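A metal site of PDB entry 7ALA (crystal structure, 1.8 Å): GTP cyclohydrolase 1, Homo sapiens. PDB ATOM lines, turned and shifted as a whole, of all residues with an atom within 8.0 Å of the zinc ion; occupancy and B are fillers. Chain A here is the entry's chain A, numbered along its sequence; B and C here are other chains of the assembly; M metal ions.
The side-chain sulfur of Cys 100 sits close to the backbone NH of His 102, at 3.5 Å. N of Cys 100 sits at hydrogen-bond distance from O of Val 105, at 2.9 Å.
Of the 17 residues printed, 3 come within 4 Å of the zinc ion. Along chain A the residues within 4 Å of the zinc ion span positions 100 to 171.
The zinc ion is bound by the side-chain sulfur of Cys 100 (2.2 Å), a ring nitrogen (ND1) of His 103 (2.2 Å) and the side-chain sulfur of Cys 171 (2.5 Å). The zinc ion has three donor atoms within binding distance.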
ATOM      1  N   MET A  99      -2.585 -27.662 -12.782  1.00  0.00           N
ATOM      2  CA  MET A  99      -1.571 -26.637 -12.808  1.00  0.00           C
ATOM      3  C   MET A  99      -1.263 -26.273 -11.370  1.00  0.00           C
ATOM      4  O   MET A  99      -2.173 -26.000 -10.600  1.00  0.00           O
ATOM      5  CB  MET A  99      -2.131 -25.376 -13.528  1.00  0.00           C
ATOM      6  CG  MET A  99      -1.092 -24.323 -13.789  1.00  0.00           C
ATOM      7  SD  MET A  99       0.214 -24.776 -14.989  1.00  0.00           S
ATOM      8  CE  MET A  99      -0.758 -25.425 -16.308  1.00  0.00           C
ATOM      9  N   CYS A 100       0.018 -26.273 -11.009  1.00  0.00           N
ATOM     10  CA  CYS A 100       0.411 -25.915  -9.647  1.00  0.00           C
ATOM     11  C   CYS A 100       0.110 -24.428  -9.430  1.00  0.00           C
ATOM     12  O   CYS A 100       0.585 -23.600 -10.192  1.00  0.00           O
ATOM     13  CB  CYS A 100       1.885 -26.221  -9.421  1.00  0.00           C
ATOM     14  SG  CYS A 100       2.485 -25.682  -7.810  1.00  0.00           S
ATOM     15  N   GLU A 101      -0.680 -24.080  -8.411  1.00  0.00           N
ATOM     16  CA  GLU A 101      -1.009 -22.687  -8.114  1.00  0.00           C
ATOM     17  C   GLU A 101       0.172 -21.882  -7.573  1.00  0.00           C
ATOM     18  O   GLU A 101       0.142 -20.663  -7.639  1.00  0.00           O
ATOM     19  CB  GLU A 101      -2.201 -22.582  -7.168  1.00  0.00           C
ATOM     20  CG  GLU A 101      -1.889 -22.972  -5.739  1.00  0.00           C
ATOM     21  CD  GLU A 101      -2.997 -22.644  -4.758  1.00  0.00           C
ATOM     22  OE1 GLU A 101      -2.706 -22.508  -3.553  1.00  0.00           O
ATOM     23  OE2 GLU A 101      -4.164 -22.533  -5.222  1.00  0.00           O
ATOM     24  N   HIS A 102       1.214 -22.540  -7.050  1.00  0.00           N
ATOM     25  CA  HIS A 102       2.388 -21.854  -6.527  1.00  0.00           C
ATOM     26  C   HIS A 102       3.386 -21.443  -7.597  1.00  0.00           C
ATOM     27  O   HIS A 102       3.940 -20.363  -7.507  1.00  0.00           O
ATOM     28  CB  HIS A 102       3.095 -22.728  -5.491  1.00  0.00           C
ATOM     29  CG  HIS A 102       2.243 -23.094  -4.326  1.00  0.00           C
ATOM     30  ND1 HIS A 102       2.304 -24.346  -3.755  1.00  0.00           N
ATOM     31  CD2 HIS A 102       1.318 -22.351  -3.673  1.00  0.00           C
ATOM     32  CE1 HIS A 102       1.424 -24.334  -2.775  1.00  0.00           C
ATOM     33  NE2 HIS A 102       0.806 -23.156  -2.689  1.00  0.00           N
ATOM     34  N   HIS A 103       3.629 -22.307  -8.602  1.00  0.00           N
ATOM     35  CA  HIS A 103       4.650 -22.026  -9.610  1.00  0.00           C
ATOM     36  C   HIS A 103       4.145 -21.904 -11.044  1.00  0.00           C
ATOM     37  O   HIS A 103       4.943 -21.587 -11.909  1.00  0.00           O
ATOM     38  CB  HIS A 103       5.744 -23.110  -9.576  1.00  0.00           C
ATOM     39  CG  HIS A 103       6.397 -23.284  -8.253  1.00  0.00           C
ATOM     40  ND1 HIS A 103       5.969 -24.248  -7.364  1.00  0.00           N
ATOM     41  CD2 HIS A 103       7.439 -22.612  -7.713  1.00  0.00           C
ATOM     42  CE1 HIS A 103       6.754 -24.128  -6.308  1.00  0.00           C
ATOM     43  NE2 HIS A 103       7.655 -23.164  -6.467  1.00  0.00           N
ATOM     44  N   LEU A 104       2.862 -22.208 -11.306  1.00  0.00           N
ATOM     45  CA  LEU A 104       2.242 -22.205 -12.625  1.00  0.00           C
ATOM     46  C   LEU A 104       2.905 -23.185 -13.596  1.00  0.00           C
ATOM     47  O   LEU A 104       3.058 -22.900 -14.789  1.00  0.00           O
ATOM     48  CB  LEU A 104       2.147 -20.793 -13.226  1.00  0.00           C
ATOM     49  CG  LEU A 104       1.436 -19.763 -12.368  1.00  0.00           C
ATOM     50  CD1 LEU A 104       1.432 -18.406 -13.047  1.00  0.00           C
ATOM     51  CD2 LEU A 104       0.027 -20.214 -12.049  1.00  0.00           C
ATOM     52  N   VAL A 105       3.307 -24.342 -13.071  1.00  0.00           N
ATOM     53  CA  VAL A 105       3.927 -25.457 -13.807  1.00  0.00           C
ATOM     54  C   VAL A 105       2.978 -26.636 -13.632  1.00  0.00           C
ATOM     55  O   VAL A 105       2.433 -26.812 -12.539  1.00  0.00           O
ATOM     56  CB  VAL A 105       5.341 -25.840 -13.240  1.00  0.00           C
ATOM     57  CG1 VAL A 105       6.110 -26.674 -14.244  1.00  0.00           C
ATOM     58  CG2 VAL A 105       6.166 -24.608 -12.897  1.00  0.00           C
ATOM     59  N   PRO A 106       2.759 -27.470 -14.672  1.00  0.00           N
ATOM     60  CA  PRO A 106       1.816 -28.592 -14.498  1.00  0.00           C
ATOM     61  C   PRO A 106       2.214 -29.692 -13.506  1.00  0.00           C
ATOM     62  O   PRO A 106       3.387 -29.974 -13.277  1.00  0.00           O
ATOM     63  CB  PRO A 106       1.709 -29.189 -15.910  1.00  0.00           C
ATOM     64  CG  PRO A 106       2.236 -28.145 -16.819  1.00  0.00           C
ATOM     65  CD  PRO A 106       3.276 -27.408 -16.053  1.00  0.00           C
ATOM     66  N   PHE A 107       1.190 -30.288 -12.902  1.00  0.00           N
ATOM     67  CA  PHE A 107       1.329 -31.507 -12.138  1.00  0.00           C
ATOM     68  C   PHE A 107       0.358 -32.450 -12.794  1.00  0.00           C
ATOM     69  O   PHE A 107      -0.780 -32.067 -13.098  1.00  0.00           O
ATOM     70  CB  PHE A 107       1.186 -31.356 -10.608  1.00  0.00           C
ATOM     71  CG  PHE A 107      -0.141 -30.994 -10.007  1.00  0.00           C
ATOM     72  CD1 PHE A 107      -0.502 -29.664  -9.837  1.00  0.00           C
ATOM     73  CD2 PHE A 107      -0.962 -31.968  -9.476  1.00  0.00           C
ATOM     74  CE1 PHE A 107      -1.690 -29.318  -9.178  1.00  0.00           C
ATOM     75  CE2 PHE A 107      -2.156 -31.620  -8.834  1.00  0.00           C
ATOM     76  CZ  PHE A 107      -2.518 -30.302  -8.690  1.00  0.00           C
ATOM     77  N   GLN A 139      -4.166 -25.180  -8.783  1.00  0.00           N
ATOM     78  CA  GLN A 139      -4.457 -26.058  -7.680  1.00  0.00           C
ATOM     79  C   GLN A 139      -3.270 -26.494  -6.824  1.00  0.00           C
ATOM     80  O   GLN A 139      -2.107 -26.252  -7.165  1.00  0.00           O
ATOM     81  CB  GLN A 139      -5.090 -27.328  -8.310  1.00  0.00           C
ATOM     82  CG  GLN A 139      -6.577 -27.189  -8.626  1.00  0.00           C
ATOM     83  CD  GLN A 139      -7.456 -27.397  -7.414  1.00  0.00           C
ATOM     84  OE1 GLN A 139      -7.017 -27.356  -6.263  1.00  0.00           O
ATOM     85  NE2 GLN A 139      -8.715 -27.647  -7.653  1.00  0.00           N
ATOM     86  N   VAL A 140      -3.582 -27.115  -5.669  1.00  0.00           N
ATOM     87  CA  VAL A 140      -2.698 -27.884  -4.804  1.00  0.00           C
ATOM     88  C   VAL A 140      -3.379 -29.263  -4.772  1.00  0.00           C
ATOM     89  O   VAL A 140      -4.615 -29.348  -4.720  1.00  0.00           O
ATOM     90  CB  VAL A 140      -2.411 -27.327  -3.371  1.00  0.00           C
ATOM     91  CG1 VAL A 140      -1.627 -26.022  -3.451  1.00  0.00           C
ATOM     92  CG2 VAL A 140      -3.685 -27.124  -2.580  1.00  0.00           C
ATOM     93  N   HIS A 169       4.992 -33.632  -9.970  1.00  0.00           N
ATOM     94  CA  HIS A 169       4.982 -32.177  -9.983  1.00  0.00           C
ATOM     95  C   HIS A 169       6.205 -31.661 -10.765  1.00  0.00           C
ATOM     96  O   HIS A 169       7.313 -31.829 -10.299  1.00  0.00           O
ATOM     97  CB  HIS A 169       5.020 -31.646  -8.542  1.00  0.00           C
ATOM     98  CG  HIS A 169       3.702 -31.688  -7.846  1.00  0.00           C
ATOM     99  ND1 HIS A 169       3.131 -32.884  -7.448  1.00  0.00           N
ATOM    100  CD2 HIS A 169       2.861 -30.677  -7.531  1.00  0.00           C
ATOM    101  CE1 HIS A 169       1.982 -32.562  -6.887  1.00  0.00           C
ATOM    102  NE2 HIS A 169       1.774 -31.247  -6.906  1.00  0.00           N
ATOM    103  N   MET A 170       5.997 -30.994 -11.907  1.00  0.00           N
ATOM    104  CA  MET A 170       7.121 -30.501 -12.722  1.00  0.00           C
ATOM    105  C   MET A 170       7.984 -29.466 -11.996  1.00  0.00           C
ATOM    106  O   MET A 170       9.147 -29.293 -12.345  1.00  0.00           O
ATOM    107  CB  MET A 170       6.655 -29.976 -14.083  1.00  0.00           C
ATOM    108  CG  MET A 170       5.889 -31.001 -14.900  1.00  0.00           C
ATOM    109  SD  MET A 170       6.965 -32.299 -15.512  1.00  0.00           S
ATOM    110  CE  MET A 170       6.047 -33.743 -15.041  1.00  0.00           C
ATOM    111  N   CYS A 171       7.422 -28.777 -10.988  1.00  0.00           N
ATOM    112  CA  CYS A 171       8.164 -27.788 -10.216  1.00  0.00           C
ATOM    113  C   CYS A 171       9.107 -28.543  -9.297  1.00  0.00           C
ATOM    114  O   CYS A 171       9.783 -27.938  -8.468  1.00  0.00           O
ATOM    115  CB  CYS A 171       7.203 -26.897  -9.425  1.00  0.00           C
ATOM    116  SG  CYS A 171       6.120 -27.827  -8.301  1.00  0.00           S
ATOM    117  N   LEU B 124       5.744 -29.773  -0.236  1.00  0.00           N
ATOM    118  CA  LEU B 124       6.284 -30.993  -0.856  1.00  0.00           C
ATOM    119  C   LEU B 124       7.807 -30.989  -0.963  1.00  0.00           C
ATOM    120  O   LEU B 124       8.433 -31.993  -0.608  1.00  0.00           O
ATOM    121  CB  LEU B 124       5.603 -31.314  -2.205  1.00  0.00           C
ATOM    122  CG  LEU B 124       5.835 -30.391  -3.442  1.00  0.00           C
ATOM    123  CD1 LEU B 124       5.861 -31.191  -4.723  1.00  0.00           C
ATOM    124  CD2 LEU B 124       4.770 -29.257  -3.536  1.00  0.00           C
ATOM    125  N   ARG C  56       7.223 -16.766  -7.504  1.00  0.00           N
ATOM    126  CA  ARG C  56       7.613 -18.179  -7.578  1.00  0.00           C
ATOM    127  C   ARG C  56       7.604 -18.648  -9.054  1.00  0.00           C
ATOM    128  O   ARG C  56       8.533 -19.350  -9.456  1.00  0.00           O
ATOM    129  CB  ARG C  56       6.689 -19.062  -6.730  1.00  0.00           C
ATOM    130  CG  ARG C  56       6.857 -18.874  -5.237  1.00  0.00           C
ATOM    131  CD  ARG C  56       5.926 -19.766  -4.432  1.00  0.00           C
ATOM    132  NE  ARG C  56       4.517 -19.394  -4.618  1.00  0.00           N
ATOM    133  CZ  ARG C  56       3.596 -19.421  -3.658  1.00  0.00           C
ATOM    134  NH1 ARG C  56       2.343 -19.050  -3.909  1.00  0.00           N
ATOM    135  NH2 ARG C  56       3.923 -19.816  -2.427  1.00  0.00           N
ATOM    136  N   ALA C  60      10.895 -19.748 -11.153  1.00  0.00           N
ATOM    137  CA  ALA C  60      10.857 -21.062 -11.768  1.00  0.00           C
ATOM    138  C   ALA C  60      11.194 -20.943 -13.255  1.00  0.00           C
ATOM    139  O   ALA C  60      12.122 -21.611 -13.703  1.00  0.00           O
ATOM    140  CB  ALA C  60       9.480 -21.712 -11.572  1.00  0.00           C
HETATM  141 ZN    ZN M   1       4.623 -25.951  -7.535  1.00  0.00          ZN
